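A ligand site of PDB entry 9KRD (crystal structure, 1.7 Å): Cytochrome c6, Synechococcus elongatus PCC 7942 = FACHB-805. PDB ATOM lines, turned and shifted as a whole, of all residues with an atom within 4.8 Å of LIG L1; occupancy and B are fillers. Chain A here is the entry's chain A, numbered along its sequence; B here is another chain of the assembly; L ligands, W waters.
The side-chain hydroxyl (OG1) of Thr 32 lies within hydrogen-bond range of the side-chain carboxylate (OD2) of Asp 37, at 2.7 Å.
The backbone NH (N) of Met 43 is in hydrogen-bond range of the backbone carbonyl oxygen (O) of Leu 38.
The side-chain amide oxygen (OD1) of Asn 25 is in hydrogen-bond range of the backbone NH (N) of Val 27 of chain A.
The side-chain amide nitrogen of Asn 25 lies within hydrogen-bond range of the backbone carbonyl oxygen of Lys 31 (2.9 Å).
The backbone NH of Asn 28 lies within hydrogen-bond range of the side-chain amide oxygen of Asn 25 (3.0 Å).
The backbone NH of Phe 63 is in hydrogen-bond range of the backbone carbonyl oxygen of Val 53 (2.8 Å).
The side-chain sulfur of Cys 16 is covalently linked to a carbon (C18) of LIG L1 (1.8 Å).
The side-chain sulfur of Met 60 is bound to an iron atom (FE1) of LIG L1 (2.4 Å).
The side-chain amino group of Lys 31 is in salt-bridge range of an oxygen (O3) of LIG L1 (2.8 Å).
A ring nitrogen (NE2) of His 20 binds an iron atom (FE1) of LIG L1, at 2.0 Å.
O of Thr 32 lies close to O1 of LIG L1.
SG of Cys 19 is bonded to C25 of LIG L1, at 1.8 Å.
Merely in contact with LIG L1: Ala 59 of chain B (2.9 Å), Gln 52 (3.2 Å), Asn 25 (3.2 Å), Val 53 (3.3 Å), Leu 33 (3.4 Å), Lys 57 (3.5 Å), Asn 15 (3.5 Å), Asp 37 (3.5 Å), Pro 61 (3.5 Å), Met 43 (3.5 Å), Tyr 41 (3.6 Å), Val 27 of chain A (3.7 Å), Ala 59 of chain A (3.7 Å), Leu 38 (3.8 Å), Ile 49 (3.8 Å), Phe 63 (3.9 Å) and Gly 58 (3.9 Å).
Water W2 lies within hydrogen-bond range of an oxygen (O3) of LIG L1 (2.5 Å) and the side-chain amide nitrogen of Gln 52 (2.7 Å).
Water W1 lies within hydrogen-bond range of O4 of LIG L1 (2.7 Å) and N of Ala 59 of chain A (2.9 Å).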
ATOM      1  N   PHE A  12      14.464  18.562  12.215  1.00  0.00           N
ATOM      2  CA  PHE A  12      13.456  17.531  11.932  1.00  0.00           C
ATOM      3  C   PHE A  12      13.784  16.762  10.657  1.00  0.00           C
ATOM      4  O   PHE A  12      13.726  15.531  10.621  1.00  0.00           O
ATOM      5  CB  PHE A  12      12.060  18.155  11.837  1.00  0.00           C
ATOM      6  CG  PHE A  12      10.958  17.127  11.774  1.00  0.00           C
ATOM      7  CD1 PHE A  12      10.425  16.600  12.947  1.00  0.00           C
ATOM      8  CD2 PHE A  12      10.485  16.669  10.555  1.00  0.00           C
ATOM      9  CE1 PHE A  12       9.427  15.625  12.894  1.00  0.00           C
ATOM     10  CE2 PHE A  12       9.490  15.711  10.485  1.00  0.00           C
ATOM     11  CZ  PHE A  12       8.957  15.175  11.660  1.00  0.00           C
ATOM     12  N   ASN A  15      16.880  14.424  11.157  1.00  0.00           N
ATOM     13  CA  ASN A  15      16.875  13.433  12.230  1.00  0.00           C
ATOM     14  C   ASN A  15      15.576  12.690  12.436  1.00  0.00           C
ATOM     15  O   ASN A  15      15.603  11.623  13.071  1.00  0.00           O
ATOM     16  CB  ASN A  15      17.240  14.106  13.563  1.00  0.00           C
ATOM     17  CG  ASN A  15      18.640  14.643  13.551  1.00  0.00           C
ATOM     18  OD1 ASN A  15      19.596  13.889  13.729  1.00  0.00           O
ATOM     19  ND2 ASN A  15      18.767  15.941  13.309  1.00  0.00           N
ATOM     20  N   CYS A  16      14.437  13.228  11.997  1.00  0.00           N
ATOM     21  CA  CYS A  16      13.142  12.666  12.342  1.00  0.00           C
ATOM     22  C   CYS A  16      12.325  12.240  11.142  1.00  0.00           C
ATOM     23  O   CYS A  16      11.498  11.330  11.257  1.00  0.00           O
ATOM     24  CB  CYS A  16      12.316  13.694  13.138  1.00  0.00           C
ATOM     25  SG  CYS A  16      13.265  14.631  14.393  1.00  0.00           S
ATOM     26  N   ALA A  18      12.959  10.458   8.702  1.00  0.00           N
ATOM     27  CA  ALA A  18      13.101   9.080   8.272  1.00  0.00           C
ATOM     28  C   ALA A  18      11.942   8.219   8.750  1.00  0.00           C
ATOM     29  O   ALA A  18      11.612   7.214   8.110  1.00  0.00           O
ATOM     30  CB  ALA A  18      14.423   8.505   8.776  1.00  0.00           C
ATOM     31  N   CYS A  19      11.317   8.590   9.878  1.00  0.00           N
ATOM     32  CA  CYS A  19      10.188   7.861  10.406  1.00  0.00           C
ATOM     33  C   CYS A  19       8.923   8.692  10.523  1.00  0.00           C
ATOM     34  O   CYS A  19       7.826   8.107  10.591  1.00  0.00           O
ATOM     35  CB  CYS A  19      10.523   7.272  11.799  1.00  0.00           C
ATOM     36  SG  CYS A  19      11.996   6.262  11.796  1.00  0.00           S
ATOM     37  N   HIS A  20       9.017  10.020  10.483  1.00  0.00           N
ATOM     38  CA  HIS A  20       7.884  10.888  10.787  1.00  0.00           C
ATOM     39  C   HIS A  20       7.608  11.902   9.685  1.00  0.00           C
ATOM     40  O   HIS A  20       7.025  12.958   9.945  1.00  0.00           O
ATOM     41  CB  HIS A  20       8.114  11.660  12.109  1.00  0.00           C
ATOM     42  CG  HIS A  20       8.214  10.803  13.341  1.00  0.00           C
ATOM     43  ND1 HIS A  20       7.185  10.012  13.810  1.00  0.00           N
ATOM     44  CD2 HIS A  20       9.209  10.695  14.261  1.00  0.00           C
ATOM     45  CE1 HIS A  20       7.541   9.444  14.952  1.00  0.00           C
ATOM     46  NE2 HIS A  20       8.766   9.847  15.246  1.00  0.00           N
ATOM     47  N   ASN A  25       4.002   8.218  11.439  1.00  0.00           N
ATOM     48  CA  ASN A  25       4.927   7.346  12.154  1.00  0.00           C
ATOM     49  C   ASN A  25       4.914   6.031  11.378  1.00  0.00           C
ATOM     50  O   ASN A  25       3.988   5.232  11.542  1.00  0.00           O
ATOM     51  CB  ASN A  25       4.547   7.144  13.619  1.00  0.00           C
ATOM     52  CG  ASN A  25       5.591   6.340  14.368  1.00  0.00           C
ATOM     53  OD1 ASN A  25       6.366   5.602  13.755  1.00  0.00           O
ATOM     54  ND2 ASN A  25       5.666   6.500  15.693  1.00  0.00           N
ATOM     55  N   VAL A  27       6.846   3.550  11.601  1.00  0.00           N
ATOM     56  CA  VAL A  27       7.227   2.373  12.391  1.00  0.00           C
ATOM     57  C   VAL A  27       6.080   1.896  13.267  1.00  0.00           C
ATOM     58  O   VAL A  27       5.743   0.704  13.281  1.00  0.00           O
ATOM     59  CB  VAL A  27       8.471   2.702  13.242  1.00  0.00           C
ATOM     60  CG1 VAL A  27       8.771   1.541  14.170  1.00  0.00           C
ATOM     61  CG2 VAL A  27       9.669   3.012  12.346  1.00  0.00           C
ATOM     62  N   ASN A  28       5.481   2.798  14.038  1.00  0.00           N
ATOM     63  CA  ASN A  28       4.338   2.490  14.890  1.00  0.00           C
ATOM     64  C   ASN A  28       3.201   3.394  14.446  1.00  0.00           C
ATOM     65  O   ASN A  28       3.083   4.537  14.921  1.00  0.00           O
ATOM     66  CB  ASN A  28       4.678   2.683  16.370  1.00  0.00           C
ATOM     67  CG  ASN A  28       3.542   2.253  17.277  1.00  0.00           C
ATOM     68  OD1 ASN A  28       2.400   2.117  16.834  1.00  0.00           O
ATOM     69  ND2 ASN A  28       3.850   2.047  18.550  1.00  0.00           N
ATOM     70  N   LYS A  31       1.141   5.859  16.727  1.00  0.00           N
ATOM     71  CA  LYS A  31       1.725   6.952  17.494  1.00  0.00           C
ATOM     72  C   LYS A  31       2.330   7.998  16.575  1.00  0.00           C
ATOM     73  O   LYS A  31       3.540   8.229  16.570  1.00  0.00           O
ATOM     74  CB  LYS A  31       2.773   6.384  18.452  1.00  0.00           C
ATOM     75  CG  LYS A  31       2.123   5.497  19.507  1.00  0.00           C
ATOM     76  CD  LYS A  31       3.104   4.969  20.520  1.00  0.00           C
ATOM     77  CE  LYS A  31       2.359   4.244  21.622  1.00  0.00           C
ATOM     78  NZ  LYS A  31       3.297   3.651  22.614  1.00  0.00           N
ATOM     79  N   THR A  32       1.475   8.651  15.780  1.00  0.00           N
ATOM     80  CA  THR A  32       1.926   9.661  14.841  1.00  0.00           C
ATOM     81  C   THR A  32       2.146  10.985  15.552  1.00  0.00           C
ATOM     82  O   THR A  32       1.959  11.112  16.767  1.00  0.00           O
ATOM     83  CB  THR A  32       0.915   9.870  13.710  1.00  0.00           C
ATOM     84  OG1 THR A  32      -0.217  10.612  14.203  1.00  0.00           O
ATOM     85  CG2 THR A  32       0.440   8.511  13.144  1.00  0.00           C
ATOM     86  N   LEU A  33       2.553  11.988  14.782  1.00  0.00           N
ATOM     87  CA  LEU A  33       2.717  13.327  15.311  1.00  0.00           C
ATOM     88  C   LEU A  33       1.495  14.191  15.031  1.00  0.00           C
ATOM     89  O   LEU A  33       1.556  15.407  15.198  1.00  0.00           O
ATOM     90  CB  LEU A  33       3.987  13.981  14.762  1.00  0.00           C
ATOM     91  CG  LEU A  33       5.257  13.130  14.799  1.00  0.00           C
ATOM     92  CD1 LEU A  33       6.453  13.967  14.351  1.00  0.00           C
ATOM     93  CD2 LEU A  33       5.490  12.574  16.210  1.00  0.00           C
ATOM     94  N   ASP A  37      -3.144  12.064  18.198  1.00  0.00           N
ATOM     95  CA  ASP A  37      -2.255  11.062  18.771  1.00  0.00           C
ATOM     96  C   ASP A  37      -1.393  11.652  19.877  1.00  0.00           C
ATOM     97  O   ASP A  37      -1.243  11.039  20.948  1.00  0.00           O
ATOM     98  CB  ASP A  37      -1.391  10.435  17.683  1.00  0.00           C
ATOM     99  CG  ASP A  37      -2.136   9.389  16.848  1.00  0.00           C
ATOM    100  OD1 ASP A  37      -3.297   9.056  17.162  1.00  0.00           O
ATOM    101  OD2 ASP A  37      -1.534   8.902  15.862  1.00  0.00           O
ATOM    102  N   LEU A  38      -0.804  12.836  19.657  1.00  0.00           N
ATOM    103  CA  LEU A  38      -0.034  13.462  20.738  1.00  0.00           C
ATOM    104  C   LEU A  38      -0.896  13.620  21.978  1.00  0.00           C
ATOM    105  O   LEU A  38      -0.436  13.365  23.102  1.00  0.00           O
ATOM    106  CB  LEU A  38       0.525  14.815  20.291  1.00  0.00           C
ATOM    107  CG  LEU A  38       1.508  14.754  19.125  1.00  0.00           C
ATOM    108  CD1 LEU A  38       2.028  16.139  18.788  1.00  0.00           C
ATOM    109  CD2 LEU A  38       2.665  13.826  19.444  1.00  0.00           C
ATOM    110  N   TYR A  41      -1.568  10.274  24.000  1.00  0.00           N
ATOM    111  CA  TYR A  41      -0.452   9.692  24.733  1.00  0.00           C
ATOM    112  C   TYR A  41       0.268  10.706  25.613  1.00  0.00           C
ATOM    113  O   TYR A  41       1.326  10.385  26.174  1.00  0.00           O
ATOM    114  CB  TYR A  41       0.517   9.026  23.756  1.00  0.00           C
ATOM    115  CG  TYR A  41      -0.160   7.935  22.948  1.00  0.00           C
ATOM    116  CD1 TYR A  41      -0.599   6.760  23.573  1.00  0.00           C
ATOM    117  CD2 TYR A  41      -0.379   8.071  21.579  1.00  0.00           C
ATOM    118  CE1 TYR A  41      -1.226   5.745  22.838  1.00  0.00           C
ATOM    119  CE2 TYR A  41      -1.001   7.077  20.849  1.00  0.00           C
ATOM    120  CZ  TYR A  41      -1.422   5.915  21.483  1.00  0.00           C
ATOM    121  OH  TYR A  41      -2.035   4.920  20.749  1.00  0.00           O
ATOM    122  N   MET A  43       1.724  13.579  24.838  1.00  0.00           N
ATOM    123  CA  MET A  43       2.944  14.046  24.215  1.00  0.00           C
ATOM    124  C   MET A  43       2.793  15.420  23.592  1.00  0.00           C
ATOM    125  O   MET A  43       3.689  15.874  22.868  1.00  0.00           O
ATOM    126  CB  MET A  43       3.405  13.015  23.163  1.00  0.00           C
ATOM    127  CG  MET A  43       3.796  11.677  23.755  1.00  0.00           C
ATOM    128  SD  MET A  43       5.269  11.867  24.771  1.00  0.00           S
ATOM    129  CE  MET A  43       6.445  12.378  23.553  1.00  0.00           C
ATOM    130  N   ILE A  49       7.808  16.062  24.459  1.00  0.00           N
ATOM    131  CA  ILE A  49       8.554  15.766  23.244  1.00  0.00           C
ATOM    132  C   ILE A  49      10.054  15.790  23.523  1.00  0.00           C
ATOM    133  O   ILE A  49      10.800  14.936  23.044  1.00  0.00           O
ATOM    134  CB  ILE A  49       8.180  16.767  22.133  1.00  0.00           C
ATOM    135  CG1 ILE A  49       6.707  16.606  21.724  1.00  0.00           C
ATOM    136  CG2 ILE A  49       9.106  16.587  20.930  1.00  0.00           C
ATOM    137  CD1 ILE A  49       6.196  17.755  20.851  1.00  0.00           C
ATOM    138  N   GLN A  52      11.179  12.546  25.175  1.00  0.00           N
ATOM    139  CA  GLN A  52      11.228  11.384  24.296  1.00  0.00           C
ATOM    140  C   GLN A  52      12.360  11.486  23.281  1.00  0.00           C
ATOM    141  O   GLN A  52      13.023  10.495  22.985  1.00  0.00           O
ATOM    142  CB  GLN A  52       9.895  11.185  23.590  1.00  0.00           C
ATOM    143  CG  GLN A  52       9.875   9.855  22.844  1.00  0.00           C
ATOM    144  CD  GLN A  52       8.562   9.160  22.979  1.00  0.00           C
ATOM    145  OE1 GLN A  52       7.945   9.172  24.046  1.00  0.00           O
ATOM    146  NE2 GLN A  52       8.105   8.526  21.903  1.00  0.00           N
ATOM    147  N   VAL A  53      12.585  12.686  22.742  1.00  0.00           N
ATOM    148  CA  VAL A  53      13.729  12.885  21.853  1.00  0.00           C
ATOM    149  C   VAL A  53      15.031  12.621  22.589  1.00  0.00           C
ATOM    150  O   VAL A  53      15.950  11.990  22.047  1.00  0.00           O
ATOM    151  CB  VAL A  53      13.675  14.309  21.269  1.00  0.00           C
ATOM    152  CG1 VAL A  53      14.947  14.630  20.480  1.00  0.00           C
ATOM    153  CG2 VAL A  53      12.445  14.431  20.378  1.00  0.00           C
ATOM    154  N   LYS A  57      12.502   5.850  23.071  1.00  0.00           N
ATOM    155  CA  LYS A  57      11.444   5.031  23.658  1.00  0.00           C
ATOM    156  C   LYS A  57      11.072   3.912  22.701  1.00  0.00           C
ATOM    157  O   LYS A  57      10.723   4.172  21.547  1.00  0.00           O
ATOM    158  CB  LYS A  57      10.189   5.847  23.960  1.00  0.00           C
ATOM    159  CG  LYS A  57       9.068   4.997  24.543  1.00  0.00           C
ATOM    160  CD  LYS A  57       7.875   5.838  24.970  1.00  0.00           C
ATOM    161  CE  LYS A  57       6.887   5.000  25.766  1.00  0.00           C
ATOM    162  NZ  LYS A  57       5.689   5.780  26.195  1.00  0.00           N
ATOM    163  N   GLY A  58      11.133   2.669  23.162  1.00  0.00           N
ATOM    164  CA  GLY A  58      10.762   1.565  22.284  1.00  0.00           C
ATOM    165  C   GLY A  58      11.648   1.544  21.061  1.00  0.00           C
ATOM    166  O   GLY A  58      12.881   1.580  21.153  1.00  0.00           O
ATOM    167  N   ALA A  59      11.027   1.503  19.892  1.00  0.00           N
ATOM    168  CA  ALA A  59      11.759   1.514  18.635  1.00  0.00           C
ATOM    169  C   ALA A  59      12.263   2.909  18.247  1.00  0.00           C
ATOM    170  O   ALA A  59      13.007   3.004  17.260  1.00  0.00           O
ATOM    171  CB  ALA A  59      10.882   0.977  17.493  1.00  0.00           C
ATOM    172  N   MET A  60      11.904   3.965  18.964  1.00  0.00           N
ATOM    173  CA  MET A  60      12.438   5.292  18.642  1.00  0.00           C
ATOM    174  C   MET A  60      13.807   5.495  19.268  1.00  0.00           C
ATOM    175  O   MET A  60      13.941   5.360  20.488  1.00  0.00           O
ATOM    176  CB  MET A  60      11.514   6.391  19.129  1.00  0.00           C
ATOM    177  CG  MET A  60      12.086   7.785  18.841  1.00  0.00           C
ATOM    178  SD  MET A  60      10.842   9.043  19.060  1.00  0.00           S
ATOM    179  CE  MET A  60      11.876  10.456  19.522  1.00  0.00           C
ATOM    180  N   PRO A  61      14.833   5.828  18.492  1.00  0.00           N
ATOM    181  CA  PRO A  61      16.159   6.074  19.075  1.00  0.00           C
ATOM    182  C   PRO A  61      16.201   7.293  19.983  1.00  0.00           C
ATOM    183  O   PRO A  61      15.344   8.179  19.955  1.00  0.00           O
ATOM    184  CB  PRO A  61      17.074   6.279  17.861  1.00  0.00           C
ATOM    185  CG  PRO A  61      16.199   6.224  16.632  1.00  0.00           C
ATOM    186  CD  PRO A  61      14.796   5.915  17.024  1.00  0.00           C
ATOM    187  N   PHE A  63      18.269  10.729  21.160  1.00  0.00           N
ATOM    188  CA  PHE A  63      19.080  11.765  20.546  1.00  0.00           C
ATOM    189  C   PHE A  63      19.817  12.633  21.563  1.00  0.00           C
ATOM    190  O   PHE A  63      20.520  13.568  21.162  1.00  0.00           O
ATOM    191  CB  PHE A  63      18.220  12.660  19.635  1.00  0.00           C
ATOM    192  CG  PHE A  63      17.615  11.929  18.478  1.00  0.00           C
ATOM    193  CD1 PHE A  63      16.456  11.190  18.649  1.00  0.00           C
ATOM    194  CD2 PHE A  63      18.204  11.981  17.227  1.00  0.00           C
ATOM    195  CE1 PHE A  63      15.895  10.494  17.564  1.00  0.00           C
ATOM    196  CE2 PHE A  63      17.652  11.293  16.136  1.00  0.00           C
ATOM    197  CZ  PHE A  63      16.507  10.556  16.310  1.00  0.00           C
ATOM    198  N   LEU A  67      22.283  15.514  19.757  1.00  0.00           N
ATOM    199  CA  LEU A  67      21.749  16.829  19.466  1.00  0.00           C
ATOM    200  C   LEU A  67      22.019  17.783  20.622  1.00  0.00           C
ATOM    201  O   LEU A  67      22.020  17.393  21.795  1.00  0.00           O
ATOM    202  CB  LEU A  67      20.241  16.757  19.201  1.00  0.00           C
ATOM    203  CG  LEU A  67      19.828  15.931  17.974  1.00  0.00           C
ATOM    204  CD1 LEU A  67      18.322  15.962  17.816  1.00  0.00           C
ATOM    205  CD2 LEU A  67      20.482  16.464  16.728  1.00  0.00           C
ATOM    206  N   VAL A  75      13.434  21.413  17.709  1.00  0.00           N
ATOM    207  CA  VAL A  75      12.669  20.391  16.999  1.00  0.00           C
ATOM    208  C   VAL A  75      11.359  20.089  17.736  1.00  0.00           C
ATOM    209  O   VAL A  75      10.330  19.837  17.108  1.00  0.00           O
ATOM    210  CB  VAL A  75      13.495  19.106  16.760  1.00  0.00           C
ATOM    211  CG1 VAL A  75      13.602  18.245  18.024  1.00  0.00           C
ATOM    212  CG2 VAL A  75      12.903  18.272  15.604  1.00  0.00           C
ATOM    213  N   VAL A  79       7.692  20.403  15.931  1.00  0.00           N
ATOM    214  CA  VAL A  79       6.695  19.334  15.920  1.00  0.00           C
ATOM    215  C   VAL A  79       5.363  19.837  16.449  1.00  0.00           C
ATOM    216  O   VAL A  79       4.301  19.582  15.864  1.00  0.00           O
ATOM    217  CB  VAL A  79       7.203  18.132  16.734  1.00  0.00           C
ATOM    218  CG1 VAL A  79       6.050  17.151  17.020  1.00  0.00           C
ATOM    219  CG2 VAL A  79       8.339  17.443  15.993  1.00  0.00           C
ATOM    220  N   VAL B  27      12.123   1.302   7.421  1.00  0.00           N
ATOM    221  CA  VAL B  27      12.696   2.650   7.366  1.00  0.00           C
ATOM    222  C   VAL B  27      13.560   2.839   6.126  1.00  0.00           C
ATOM    223  O   VAL B  27      13.534   3.901   5.516  1.00  0.00           O
ATOM    224  CB  VAL B  27      13.517   2.918   8.643  1.00  0.00           C
ATOM    225  CG1 VAL B  27      14.105   4.345   8.622  1.00  0.00           C
ATOM    226  CG2 VAL B  27      12.652   2.705   9.865  1.00  0.00           C
ATOM    227  N   ALA B  59      19.123   5.587  11.910  1.00  0.00           N
ATOM    228  CA  ALA B  59      17.775   5.523  12.456  1.00  0.00           C
ATOM    229  C   ALA B  59      17.502   4.260  13.247  1.00  0.00           C
ATOM    230  O   ALA B  59      16.450   4.153  13.875  1.00  0.00           O
ATOM    231  CB  ALA B  59      16.724   5.631  11.334  1.00  0.00           C
HETATM  232 FE1  LIG L   1       9.781   9.473  16.984  1.00  0.00          FE
HETATM  233  C1  LIG L   1       7.115   8.425  18.892  1.00  0.00           C
HETATM  234  C2  LIG L   1       9.226  12.694  17.934  1.00  0.00           C
HETATM  235  C3  LIG L   1      12.622  10.491  15.333  1.00  0.00           C
HETATM  236  C4  LIG L   1      10.105   6.364  15.630  1.00  0.00           C
HETATM  237  N1  LIG L   1       8.403  10.378  18.154  1.00  0.00           N
HETATM  238  C5  LIG L   1       7.350   9.777  18.811  1.00  0.00           C
HETATM  239  C6  LIG L   1       6.559  10.819  19.420  1.00  0.00           C
HETATM  240  C7  LIG L   1       7.141  12.007  19.168  1.00  0.00           C
HETATM  241  C8  LIG L   1       8.335  11.749  18.389  1.00  0.00           C
HETATM  242  C9  LIG L   1       6.647  13.389  19.628  1.00  0.00           C
HETATM  243  C10 LIG L   1       5.251  10.590  20.211  1.00  0.00           C
HETATM  244  C11 LIG L   1       4.123  10.358  19.179  1.00  0.00           C
HETATM  245  C12 LIG L   1       2.814   9.965  19.815  1.00  0.00           C
HETATM  246  O1  LIG L   1       1.752   9.955  19.123  1.00  0.00           O
HETATM  247  O2  LIG L   1       2.813   9.655  21.031  1.00  0.00           O
HETATM  248  N2  LIG L   1      10.746  11.200  16.717  1.00  0.00           N
HETATM  249  C13 LIG L   1      10.374  12.438  17.216  1.00  0.00           C
HETATM  250  C14 LIG L   1      11.431  13.385  16.970  1.00  0.00           C
HETATM  251  C15 LIG L   1      12.344  12.798  16.186  1.00  0.00           C
HETATM  252  C16 LIG L   1      11.958  11.416  16.067  1.00  0.00           C
HETATM  253  C17 LIG L   1      11.257  14.886  17.300  1.00  0.00           C
HETATM  254  C18 LIG L   1      13.646  13.367  15.566  1.00  0.00           C
HETATM  255  C19 LIG L   1      14.567  14.029  16.621  1.00  0.00           C
HETATM  256  N3  LIG L   1      11.091   8.612  15.729  1.00  0.00           N
HETATM  257  C20 LIG L   1      12.182   9.202  15.121  1.00  0.00           C
HETATM  258  C21 LIG L   1      12.937   8.183  14.423  1.00  0.00           C
HETATM  259  C22 LIG L   1      12.152   7.091  14.339  1.00  0.00           C
HETATM  260  C23 LIG L   1      11.042   7.295  15.257  1.00  0.00           C
HETATM  261  C24 LIG L   1      14.082   8.518  13.448  1.00  0.00           C
HETATM  262  C25 LIG L   1      12.416   5.801  13.478  1.00  0.00           C
HETATM  263  C26 LIG L   1      13.674   5.032  13.824  1.00  0.00           C
HETATM  264  N4  LIG L   1       8.736   7.685  17.205  1.00  0.00           N
HETATM  265  C27 LIG L   1       9.175   6.485  16.635  1.00  0.00           C
HETATM  266  C28 LIG L   1       8.483   5.386  17.286  1.00  0.00           C
HETATM  267  C29 LIG L   1       7.551   6.027  18.294  1.00  0.00           C
HETATM  268  C30 LIG L   1       7.790   7.454  18.184  1.00  0.00           C
HETATM  269  C31 LIG L   1       8.634   3.886  17.017  1.00  0.00           C
HETATM  270  C32 LIG L   1       6.612   5.331  19.292  1.00  0.00           C
HETATM  271  C33 LIG L   1       7.509   4.959  20.476  1.00  0.00           C
HETATM  272  C34 LIG L   1       6.761   4.152  21.525  1.00  0.00           C
HETATM  273  O3  LIG L   1       5.830   4.700  22.163  1.00  0.00           O
HETATM  274  O4  LIG L   1       7.121   2.971  21.728  1.00  0.00           O
HETATM  275 FE1  LG2 L   2      17.778  -2.826  12.403  1.00  0.00          FE
HETATM  276  C1  LG2 L   2      19.926  -2.111   9.808  1.00  0.00           C
HETATM  277  C2  LG2 L   2      19.272  -5.817  12.845  1.00  0.00           C
HETATM  278  C3  LG2 L   2      15.773  -3.423  15.127  1.00  0.00           C
HETATM  279  C4  LG2 L   2      15.907  -0.059  11.663  1.00  0.00           C
HETATM  280  N1  LG2 L   2      19.291  -3.763  11.479  1.00  0.00           N
HETATM  281  C5  LG2 L   2      20.026  -3.349  10.398  1.00  0.00           C
HETATM  282  C6  LG2 L   2      20.967  -4.384  10.030  1.00  0.00           C
HETATM  283  C7  LG2 L   2      20.778  -5.413  10.866  1.00  0.00           C
HETATM  284  C8  LG2 L   2      19.734  -5.041  11.805  1.00  0.00           C
HETATM  285  C9  LG2 L   2      21.555  -6.746  10.854  1.00  0.00           C
HETATM  286  C10 LG2 L   2      21.949  -4.308   8.837  1.00  0.00           C
HETATM  287  C11 LG2 L   2      21.085  -4.580   7.587  1.00  0.00           C
HETATM  288  C12 LG2 L   2      21.852  -4.401   6.299  1.00  0.00           C
HETATM  289  O1  LG2 L   2      21.319  -4.764   5.202  1.00  0.00           O
HETATM  290  O2  LG2 L   2      23.010  -3.890   6.375  1.00  0.00           O
HETATM  291  N2  LG2 L   2      17.580  -4.278  13.730  1.00  0.00           N
HETATM  292  C13 LG2 L   2      18.315  -5.460  13.759  1.00  0.00           C
HETATM  293  C14 LG2 L   2      18.004  -6.167  14.991  1.00  0.00           C
HETATM  294  C15 LG2 L   2      16.998  -5.517  15.581  1.00  0.00           C
HETATM  295  C16 LG2 L   2      16.759  -4.310  14.832  1.00  0.00           C
HETATM  296  C17 LG2 L   2      18.553  -7.589  15.308  1.00  0.00           C
HETATM  297  C18 LG2 L   2      16.213  -5.869  16.867  1.00  0.00           C
HETATM  298  C19 LG2 L   2      17.140  -6.040  18.087  1.00  0.00           C
HETATM  299  N3  LG2 L   2      16.151  -1.932  13.215  1.00  0.00           N
HETATM  300  C20 LG2 L   2      15.454  -2.336  14.342  1.00  0.00           C
HETATM  301  C21 LG2 L   2      14.473  -1.323  14.703  1.00  0.00           C
HETATM  302  C22 LG2 L   2      14.397  -0.490  13.661  1.00  0.00           C
HETATM  303  C23 LG2 L   2      15.507  -0.792  12.764  1.00  0.00           C
HETATM  304  C24 LG2 L   2      13.384  -1.537  15.775  1.00  0.00           C
HETATM  305  C25 LG2 L   2      13.369   0.654  13.447  1.00  0.00           C
HETATM  306  C26 LG2 L   2      13.279   1.699  14.561  1.00  0.00           C
HETATM  307  N4  LG2 L   2      17.878  -1.360  10.943  1.00  0.00           N
HETATM  308  C27 LG2 L   2      17.083  -0.221  10.957  1.00  0.00           C
HETATM  309  C28 LG2 L   2      17.681   0.761  10.079  1.00  0.00           C
HETATM  310  C29 LG2 L   2      18.925   0.125   9.499  1.00  0.00           C
HETATM  311  C30 LG2 L   2      18.976  -1.183  10.097  1.00  0.00           C
HETATM  312  C31 LG2 L   2      17.151   2.166   9.778  1.00  0.00           C
HETATM  313  C32 LG2 L   2      19.960   0.738   8.544  1.00  0.00           C
HETATM  314  C33 LG2 L   2      20.846   1.633   9.432  1.00  0.00           C
HETATM  315  C34 LG2 L   2      21.859   2.395   8.613  1.00  0.00           C
HETATM  316  O3  LG2 L   2      22.751   1.771   8.002  1.00  0.00           O
HETATM  317  O4  LG2 L   2      21.756   3.653   8.585  1.00  0.00           O
HETATM  318  O   HOH W   1       8.128   1.220  19.899  1.00  0.00           O
HETATM  319  O   HOH W   2       5.741   7.209  21.969  1.00  0.00           O
HETATM  320  O   HOH W   3       3.514   7.907  23.102  1.00  0.00           O
